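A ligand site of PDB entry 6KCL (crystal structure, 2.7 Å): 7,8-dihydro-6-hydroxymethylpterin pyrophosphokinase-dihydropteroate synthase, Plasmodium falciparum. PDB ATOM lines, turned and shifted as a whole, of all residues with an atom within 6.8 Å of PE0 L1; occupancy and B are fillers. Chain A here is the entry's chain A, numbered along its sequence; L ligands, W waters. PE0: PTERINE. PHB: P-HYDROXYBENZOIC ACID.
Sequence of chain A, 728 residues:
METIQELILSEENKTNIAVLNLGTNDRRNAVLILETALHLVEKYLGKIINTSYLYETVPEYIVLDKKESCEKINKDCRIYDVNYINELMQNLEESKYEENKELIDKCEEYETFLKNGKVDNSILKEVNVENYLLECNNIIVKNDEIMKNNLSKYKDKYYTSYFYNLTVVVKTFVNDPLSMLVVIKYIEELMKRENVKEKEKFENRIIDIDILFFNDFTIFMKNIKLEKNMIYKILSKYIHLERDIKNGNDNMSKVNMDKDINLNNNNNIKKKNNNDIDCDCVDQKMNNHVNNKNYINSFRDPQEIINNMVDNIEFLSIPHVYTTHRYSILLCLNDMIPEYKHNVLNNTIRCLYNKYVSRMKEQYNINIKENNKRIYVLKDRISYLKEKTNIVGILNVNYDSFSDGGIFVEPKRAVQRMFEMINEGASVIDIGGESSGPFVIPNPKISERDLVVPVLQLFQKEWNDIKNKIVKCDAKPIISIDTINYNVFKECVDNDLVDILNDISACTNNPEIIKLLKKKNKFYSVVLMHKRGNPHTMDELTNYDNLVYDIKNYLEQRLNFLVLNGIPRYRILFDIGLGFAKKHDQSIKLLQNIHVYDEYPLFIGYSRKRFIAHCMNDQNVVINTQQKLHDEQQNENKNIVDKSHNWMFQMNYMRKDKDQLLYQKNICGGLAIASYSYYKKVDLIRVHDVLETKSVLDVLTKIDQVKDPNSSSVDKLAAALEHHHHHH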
ATOM      1  N   ILE A 394      29.221   5.190  -1.571  1.00  0.00           N
ATOM      2  CA  ILE A 394      30.488   5.891  -1.739  1.00  0.00           C
ATOM      3  C   ILE A 394      31.686   5.048  -1.304  1.00  0.00           C
ATOM      4  O   ILE A 394      31.667   4.446  -0.242  1.00  0.00           O
ATOM      5  CB  ILE A 394      30.483   7.189  -0.915  1.00  0.00           C
ATOM      6  CG1 ILE A 394      29.370   8.122  -1.399  1.00  0.00           C
ATOM      7  CG2 ILE A 394      31.850   7.847  -0.986  1.00  0.00           C
ATOM      8  CD1 ILE A 394      28.928   9.134  -0.369  1.00  0.00           C
ATOM      9  N   ASN A 396      35.475   6.289  -0.879  1.00  0.00           N
ATOM     10  CA  ASN A 396      36.551   7.277  -0.932  1.00  0.00           C
ATOM     11  C   ASN A 396      37.884   6.612  -0.628  1.00  0.00           C
ATOM     12  O   ASN A 396      38.167   6.328   0.523  1.00  0.00           O
ATOM     13  CB  ASN A 396      36.338   8.365   0.115  1.00  0.00           C
ATOM     14  CG  ASN A 396      35.159   9.265  -0.204  1.00  0.00           C
ATOM     15  OD1 ASN A 396      35.002   9.712  -1.339  1.00  0.00           O
ATOM     16  ND2 ASN A 396      34.336   9.562   0.814  1.00  0.00           N
ATOM     17  N   ASP A 430      30.386   4.129  -6.195  1.00  0.00           N
ATOM     18  CA  ASP A 430      31.046   5.332  -6.733  1.00  0.00           C
ATOM     19  C   ASP A 430      32.408   5.497  -6.089  1.00  0.00           C
ATOM     20  O   ASP A 430      32.483   5.874  -4.927  1.00  0.00           O
ATOM     21  CB  ASP A 430      30.198   6.595  -6.499  1.00  0.00           C
ATOM     22  CG  ASP A 430      30.807   7.865  -7.160  1.00  0.00           C
ATOM     23  OD1 ASP A 430      31.158   7.829  -8.365  1.00  0.00           O
ATOM     24  OD2 ASP A 430      30.942   8.923  -6.475  1.00  0.00           O
ATOM     25  N   GLU A 434      39.763  11.732  -4.783  1.00  0.00           N
ATOM     26  CA  GLU A 434      39.913  13.184  -4.550  1.00  0.00           C
ATOM     27  C   GLU A 434      38.858  13.728  -3.564  1.00  0.00           C
ATOM     28  O   GLU A 434      37.795  13.122  -3.387  1.00  0.00           O
ATOM     29  CB  GLU A 434      39.865  13.969  -5.879  1.00  0.00           C
ATOM     30  CG  GLU A 434      41.124  13.814  -6.750  1.00  0.00           C
ATOM     31  CD  GLU A 434      42.118  14.965  -6.640  1.00  0.00           C
ATOM     32  OE1 GLU A 434      42.885  15.174  -7.602  1.00  0.00           O
ATOM     33  OE2 GLU A 434      42.149  15.670  -5.599  1.00  0.00           O
ATOM     34  N   ASP A 482      34.390   8.853  -9.658  1.00  0.00           N
ATOM     35  CA  ASP A 482      34.234  10.236  -9.329  1.00  0.00           C
ATOM     36  C   ASP A 482      35.525  10.956  -9.670  1.00  0.00           C
ATOM     37  O   ASP A 482      36.393  11.099  -8.820  1.00  0.00           O
ATOM     38  CB  ASP A 482      33.967  10.352  -7.828  1.00  0.00           C
ATOM     39  CG  ASP A 482      33.579  11.749  -7.395  1.00  0.00           C
ATOM     40  OD1 ASP A 482      33.881  12.727  -8.114  1.00  0.00           O
ATOM     41  OD2 ASP A 482      32.975  11.879  -6.309  1.00  0.00           O
ATOM     42  N   ASN A 502      31.551  10.022 -13.170  1.00  0.00           N
ATOM     43  CA  ASN A 502      30.880  10.990 -12.294  1.00  0.00           C
ATOM     44  C   ASN A 502      31.734  12.243 -12.287  1.00  0.00           C
ATOM     45  O   ASN A 502      32.706  12.327 -11.527  1.00  0.00           O
ATOM     46  CB  ASN A 502      30.656  10.423 -10.885  1.00  0.00           C
ATOM     47  CG  ASN A 502      30.187  11.473  -9.894  1.00  0.00           C
ATOM     48  OD1 ASN A 502      29.650  12.515 -10.281  1.00  0.00           O
ATOM     49  ND2 ASN A 502      30.390  11.216  -8.608  1.00  0.00           N
ATOM     50  N   ASP A 503      31.384  13.213 -13.138  1.00  0.00           N
ATOM     51  CA  ASP A 503      32.221  14.414 -13.331  1.00  0.00           C
ATOM     52  C   ASP A 503      31.615  15.591 -12.559  1.00  0.00           C
ATOM     53  O   ASP A 503      30.598  16.150 -12.964  1.00  0.00           O
ATOM     54  CB  ASP A 503      32.340  14.754 -14.816  1.00  0.00           C
ATOM     55  CG  ASP A 503      33.373  15.834 -15.093  1.00  0.00           C
ATOM     56  OD1 ASP A 503      33.327  16.920 -14.442  1.00  0.00           O
ATOM     57  OD2 ASP A 503      34.240  15.628 -15.968  1.00  0.00           O
ATOM     58  N   ILE A 504      32.270  15.974 -11.464  1.00  0.00           N
ATOM     59  CA  ILE A 504      31.699  17.029 -10.605  1.00  0.00           C
ATOM     60  C   ILE A 504      31.824  18.440 -11.187  1.00  0.00           C
ATOM     61  O   ILE A 504      31.341  19.414 -10.603  1.00  0.00           O
ATOM     62  CB  ILE A 504      32.202  16.971  -9.139  1.00  0.00           C
ATOM     63  CG1 ILE A 504      33.710  17.190  -9.052  1.00  0.00           C
ATOM     64  CG2 ILE A 504      31.787  15.669  -8.480  1.00  0.00           C
ATOM     65  CD1 ILE A 504      34.088  17.856  -7.748  1.00  0.00           C
ATOM     66  N   VAL A 527      27.460  11.434 -15.067  1.00  0.00           N
ATOM     67  CA  VAL A 527      26.732  12.287 -14.142  1.00  0.00           C
ATOM     68  C   VAL A 527      27.286  13.676 -14.340  1.00  0.00           C
ATOM     69  O   VAL A 527      28.504  13.845 -14.386  1.00  0.00           O
ATOM     70  CB  VAL A 527      26.950  11.854 -12.685  1.00  0.00           C
ATOM     71  CG1 VAL A 527      26.140  12.703 -11.718  1.00  0.00           C
ATOM     72  CG2 VAL A 527      26.574  10.401 -12.518  1.00  0.00           C
ATOM     73  N   LEU A 528      26.412  14.670 -14.480  1.00  0.00           N
ATOM     74  CA  LEU A 528      26.862  16.029 -14.604  1.00  0.00           C
ATOM     75  C   LEU A 528      26.417  16.758 -13.367  1.00  0.00           C
ATOM     76  O   LEU A 528      25.204  16.880 -13.104  1.00  0.00           O
ATOM     77  CB  LEU A 528      26.188  16.664 -15.803  1.00  0.00           C
ATOM     78  CG  LEU A 528      26.491  16.110 -17.194  1.00  0.00           C
ATOM     79  CD1 LEU A 528      25.693  16.848 -18.278  1.00  0.00           C
ATOM     80  CD2 LEU A 528      28.008  16.105 -17.473  1.00  0.00           C
ATOM     81  N   MET A 529      27.371  17.260 -12.601  1.00  0.00           N
ATOM     82  CA  MET A 529      27.042  17.959 -11.369  1.00  0.00           C
ATOM     83  C   MET A 529      27.289  19.476 -11.469  1.00  0.00           C
ATOM     84  O   MET A 529      28.267  19.909 -12.076  1.00  0.00           O
ATOM     85  CB  MET A 529      27.854  17.364 -10.232  1.00  0.00           C
ATOM     86  CG  MET A 529      27.264  17.659  -8.857  1.00  0.00           C
ATOM     87  SD  MET A 529      28.438  17.501  -7.497  1.00  0.00           S
ATOM     88  CE  MET A 529      29.491  18.937  -7.746  1.00  0.00           C
ATOM     89  N   ASP A 575      22.771  16.365 -11.524  1.00  0.00           N
ATOM     90  CA  ASP A 575      23.057  16.441 -10.110  1.00  0.00           C
ATOM     91  C   ASP A 575      23.237  17.903  -9.745  1.00  0.00           C
ATOM     92  O   ASP A 575      24.069  18.608 -10.310  1.00  0.00           O
ATOM     93  CB  ASP A 575      24.298  15.633  -9.766  1.00  0.00           C
ATOM     94  CG  ASP A 575      24.590  15.595  -8.264  1.00  0.00           C
ATOM     95  OD1 ASP A 575      23.981  16.406  -7.494  1.00  0.00           O
ATOM     96  OD2 ASP A 575      25.430  14.755  -7.848  1.00  0.00           O
ATOM     97  N   ILE A 576      22.435  18.355  -8.805  1.00  0.00           N
ATOM     98  CA  ILE A 576      22.422  19.735  -8.364  1.00  0.00           C
ATOM     99  C   ILE A 576      23.656  20.132  -7.532  1.00  0.00           C
ATOM    100  O   ILE A 576      23.830  21.306  -7.211  1.00  0.00           O
ATOM    101  CB  ILE A 576      21.183  19.969  -7.506  1.00  0.00           C
ATOM    102  CG1 ILE A 576      21.049  18.824  -6.486  1.00  0.00           C
ATOM    103  CG2 ILE A 576      19.953  19.979  -8.398  1.00  0.00           C
ATOM    104  CD1 ILE A 576      19.887  18.935  -5.532  1.00  0.00           C
ATOM    105  N   GLY A 577      24.492  19.165  -7.180  1.00  0.00           N
ATOM    106  CA  GLY A 577      25.691  19.427  -6.372  1.00  0.00           C
ATOM    107  C   GLY A 577      25.412  20.059  -5.017  1.00  0.00           C
ATOM    108  O   GLY A 577      25.815  21.194  -4.752  1.00  0.00           O
ATOM    109  N   LEU A 578      24.730  19.333  -4.149  1.00  0.00           N
ATOM    110  CA  LEU A 578      24.397  19.878  -2.823  1.00  0.00           C
ATOM    111  C   LEU A 578      25.691  20.188  -2.078  1.00  0.00           C
ATOM    112  O   LEU A 578      26.637  19.377  -2.071  1.00  0.00           O
ATOM    113  CB  LEU A 578      23.564  18.879  -2.028  1.00  0.00           C
ATOM    114  CG  LEU A 578      22.145  18.594  -2.496  1.00  0.00           C
ATOM    115  CD1 LEU A 578      21.581  17.426  -1.701  1.00  0.00           C
ATOM    116  CD2 LEU A 578      21.278  19.818  -2.313  1.00  0.00           C
ATOM    117  N   GLY A 579      25.749  21.365  -1.460  1.00  0.00           N
ATOM    118  CA  GLY A 579      26.955  21.766  -0.730  1.00  0.00           C
ATOM    119  C   GLY A 579      28.138  22.335  -1.525  1.00  0.00           C
ATOM    120  O   GLY A 579      29.121  22.751  -0.933  1.00  0.00           O
ATOM    121  N   PHE A 580      28.047  22.349  -2.859  1.00  0.00           N
ATOM    122  CA  PHE A 580      29.114  22.886  -3.688  1.00  0.00           C
ATOM    123  C   PHE A 580      28.706  24.263  -4.156  1.00  0.00           C
ATOM    124  O   PHE A 580      27.909  24.405  -5.093  1.00  0.00           O
ATOM    125  CB  PHE A 580      29.297  22.043  -4.930  1.00  0.00           C
ATOM    126  CG  PHE A 580      29.930  20.704  -4.694  1.00  0.00           C
ATOM    127  CD1 PHE A 580      29.141  19.595  -4.345  1.00  0.00           C
ATOM    128  CD2 PHE A 580      31.319  20.528  -4.876  1.00  0.00           C
ATOM    129  CE1 PHE A 580      29.721  18.354  -4.151  1.00  0.00           C
ATOM    130  CE2 PHE A 580      31.907  19.275  -4.684  1.00  0.00           C
ATOM    131  CZ  PHE A 580      31.109  18.185  -4.325  1.00  0.00           C
ATOM    132  N   PHE A 603      20.413  12.390  -9.918  1.00  0.00           N
ATOM    133  CA  PHE A 603      21.424  11.790  -9.061  1.00  0.00           C
ATOM    134  C   PHE A 603      21.742  12.881  -8.022  1.00  0.00           C
ATOM    135  O   PHE A 603      22.057  14.007  -8.383  1.00  0.00           O
ATOM    136  CB  PHE A 603      22.653  11.519  -9.944  1.00  0.00           C
ATOM    137  CG  PHE A 603      23.847  10.921  -9.228  1.00  0.00           C
ATOM    138  CD1 PHE A 603      24.551  11.629  -8.247  1.00  0.00           C
ATOM    139  CD2 PHE A 603      24.302   9.655  -9.588  1.00  0.00           C
ATOM    140  CE1 PHE A 603      25.676  11.077  -7.639  1.00  0.00           C
ATOM    141  CE2 PHE A 603      25.407   9.088  -8.957  1.00  0.00           C
ATOM    142  CZ  PHE A 603      26.090   9.809  -7.978  1.00  0.00           C
ATOM    143  N   ILE A 604      21.580  12.580  -6.726  1.00  0.00           N
ATOM    144  CA  ILE A 604      21.977  13.535  -5.672  1.00  0.00           C
ATOM    145  C   ILE A 604      22.885  12.944  -4.574  1.00  0.00           C
ATOM    146  O   ILE A 604      22.897  11.729  -4.326  1.00  0.00           O
ATOM    147  CB  ILE A 604      20.773  14.247  -5.038  1.00  0.00           C
ATOM    148  CG1 ILE A 604      20.007  13.336  -4.078  1.00  0.00           C
ATOM    149  CG2 ILE A 604      19.876  14.851  -6.118  1.00  0.00           C
ATOM    150  CD1 ILE A 604      18.829  14.026  -3.406  1.00  0.00           C
ATOM    151  N   GLY A 605      23.646  13.834  -3.931  1.00  0.00           N
ATOM    152  CA  GLY A 605      24.571  13.458  -2.883  1.00  0.00           C
ATOM    153  C   GLY A 605      24.370  14.389  -1.709  1.00  0.00           C
ATOM    154  O   GLY A 605      24.863  15.530  -1.727  1.00  0.00           O
ATOM    155  N   TYR A 606      23.648  13.927  -0.691  1.00  0.00           N
ATOM    156  CA  TYR A 606      23.433  14.733   0.496  1.00  0.00           C
ATOM    157  C   TYR A 606      24.286  14.222   1.621  1.00  0.00           C
ATOM    158  O   TYR A 606      24.465  14.901   2.646  1.00  0.00           O
ATOM    159  CB  TYR A 606      21.982  14.643   0.925  1.00  0.00           C
ATOM    160  CG  TYR A 606      21.468  13.215   1.097  1.00  0.00           C
ATOM    161  CD1 TYR A 606      21.743  12.480   2.253  1.00  0.00           C
ATOM    162  CD2 TYR A 606      20.669  12.609   0.103  1.00  0.00           C
ATOM    163  CE1 TYR A 606      21.281  11.193   2.406  1.00  0.00           C
ATOM    164  CE2 TYR A 606      20.195  11.316   0.245  1.00  0.00           C
ATOM    165  CZ  TYR A 606      20.508  10.619   1.401  1.00  0.00           C
ATOM    166  OH  TYR A 606      20.044   9.339   1.561  1.00  0.00           O
ATOM    167  N   SER A 607      24.791  12.997   1.435  1.00  0.00           N
ATOM    168  CA  SER A 607      25.352  12.194   2.504  1.00  0.00           C
ATOM    169  C   SER A 607      26.494  12.864   3.294  1.00  0.00           C
ATOM    170  O   SER A 607      27.558  13.159   2.744  1.00  0.00           O
ATOM    171  CB  SER A 607      25.795  10.836   1.954  1.00  0.00           C
ATOM    172  OG  SER A 607      26.149   9.953   2.998  1.00  0.00           O
ATOM    173  N   LYS A 609      26.949  15.725   4.475  1.00  0.00           N
ATOM    174  CA  LYS A 609      27.280  17.089   4.135  1.00  0.00           C
ATOM    175  C   LYS A 609      26.837  18.016   5.253  1.00  0.00           C
ATOM    176  O   LYS A 609      25.863  17.730   5.960  1.00  0.00           O
ATOM    177  CB  LYS A 609      26.664  17.501   2.807  1.00  0.00           C
ATOM    178  CG  LYS A 609      27.134  16.639   1.639  1.00  0.00           C
ATOM    179  CD  LYS A 609      27.392  17.470   0.408  1.00  0.00           C
ATOM    180  CE  LYS A 609      28.076  16.651  -0.676  1.00  0.00           C
ATOM    181  NZ  LYS A 609      27.247  16.399  -1.880  1.00  0.00           N
ATOM    182  N   ARG A 686      23.462   9.118  -3.552  1.00  0.00           N
ATOM    183  CA  ARG A 686      24.870   8.787  -3.311  1.00  0.00           C
ATOM    184  C   ARG A 686      25.150   8.848  -1.805  1.00  0.00           C
ATOM    185  O   ARG A 686      25.170   9.925  -1.227  1.00  0.00           O
ATOM    186  CB  ARG A 686      25.751   9.775  -4.061  1.00  0.00           C
ATOM    187  CG  ARG A 686      27.226   9.434  -4.095  1.00  0.00           C
ATOM    188  CD  ARG A 686      28.038  10.506  -4.784  1.00  0.00           C
ATOM    189  NE  ARG A 686      29.465  10.278  -4.616  1.00  0.00           N
ATOM    190  CZ  ARG A 686      30.202  10.788  -3.617  1.00  0.00           C
ATOM    191  NH1 ARG A 686      31.498  10.511  -3.553  1.00  0.00           N
ATOM    192  NH2 ARG A 686      29.652  11.582  -2.686  1.00  0.00           N
HETATM  193  C1  PE0 L   1      29.239  14.619  -4.530  1.00  0.00           C
HETATM  194  C4  PE0 L   1      27.846  14.908  -4.974  1.00  0.00           C
HETATM  195  O4  PE0 L   1      27.030  15.473  -4.215  1.00  0.00           O
HETATM  196  N2  PE0 L   1      27.498  14.526  -6.211  1.00  0.00           N
HETATM  197  C3  PE0 L   1      28.350  13.901  -7.044  1.00  0.00           C
HETATM  198  N6  PE0 L   1      27.891  13.567  -8.264  1.00  0.00           N
HETATM  199  N1  PE0 L   1      29.638  13.595  -6.714  1.00  0.00           N
HETATM  200  C2  PE0 L   1      30.126  13.923  -5.495  1.00  0.00           C
HETATM  201  N3  PE0 L   1      31.409  13.657  -5.107  1.00  0.00           N
HETATM  202  C6  PE0 L   1      31.808  13.995  -3.875  1.00  0.00           C
HETATM  203  C5  PE0 L   1      30.969  14.661  -2.968  1.00  0.00           C
HETATM  204  N4  PE0 L   1      29.703  14.955  -3.296  1.00  0.00           N
HETATM  205  C1' PHB L   2      29.631  19.729   2.517  1.00  0.00           C
HETATM  206  O1' PHB L   2      29.566  19.106   3.588  1.00  0.00           O
HETATM  207  O2' PHB L   2      29.081  20.827   2.361  1.00  0.00           O
HETATM  208  C1  PHB L   2      30.431  19.156   1.400  1.00  0.00           C
HETATM  209  C2  PHB L   2      31.099  17.958   1.599  1.00  0.00           C
HETATM  210  C3  PHB L   2      31.846  17.398   0.595  1.00  0.00           C
HETATM  211  C4  PHB L   2      31.907  18.060  -0.620  1.00  0.00           C
HETATM  212  C5  PHB L   2      31.233  19.267  -0.855  1.00  0.00           C
HETATM  213  C6  PHB L   2      30.487  19.824   0.179  1.00  0.00           C
HETATM  214  O4  PHB L   2      32.643  17.508  -1.606  1.00  0.00           O
HETATM  215  O   HOH W   1      24.365  16.290  -4.965  1.00  0.00           O
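O4 of PE0 L1 lies within hydrogen-bond range of NZ of Lys 609, at 2.5 Å. The side-chain sulfur (SD) of Met 529 lies within hydrogen-bond range of a nitrogen (N2) of PE0 L1 (3.4 Å). The side-chain amide oxygen (OD1) of Asn 502 is in hydrogen-bond range of a nitrogen (N6) of PE0 L1, at 2.9 Å. OD2 of Asp 575 sits at hydrogen-bond distance from N2 of PE0 L1. A nitrogen (N4) of PE0 L1 lies close to the guanidinium group (NH2) of Arg 686. The side-chain carboxylate (OD2) of Asp 482 is in hydrogen-bond range of a nitrogen (N3) of PE0 L1, at 2.7 Å.
N of Asp 575 sits at hydrogen-bond distance from O of Leu 528. NH1 of Arg 686 is in salt-bridge range of OD2 of Asp 482, at 3.4 Å. O of Val 527 is in hydrogen-bond range of N of Asp 503 (3.2 Å). The backbone NH (N) of Met 529 sits at hydrogen-bond distance from the backbone carbonyl oxygen (O) of Asp 503. The backbone carbonyl oxygen of Gly 605 sits at hydrogen-bond distance from the side-chain amino group of Lys 609, 2.5 Å away. O of Leu 578 is in hydrogen-bond range of NZ of Lys 609. The side-chain amide nitrogen of Asn 502 lies within hydrogen-bond range of the side-chain carboxylate of Asp 430 (3.2 Å). The backbone carbonyl oxygen (O) of Ile 604 is in hydrogen-bond range of the backbone NH (N) of Arg 686 (2.8 Å).
An oxygen (O4) of PE0 L1 sits close to the backbone carbonyl oxygen of Gly 605 (3.3 Å). Merely in contact with PE0 L1: Ile 504, Val 527, Phe 580 and Phe 603. Hydrophobic or aromatic side chains within 4 Å of PE0 L1: Ile 504, Val 527, Met 529, Phe 580 and Phe 603. Of the 24 residues printed, 11 come within 4 Å of PE0 L1. The nearest printed residue that does not touch PE0 L1 is Leu 578 (4.5 Å).
Water W1 lies within hydrogen-bond range of the side-chain carboxylate of Asp 575 (2.6 Å), the backbone NH of Gly 605 (2.8 Å), an oxygen (O4) of PE0 L1 (2.9 Å) and the backbone NH of Leu 578 (3.2 Å).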
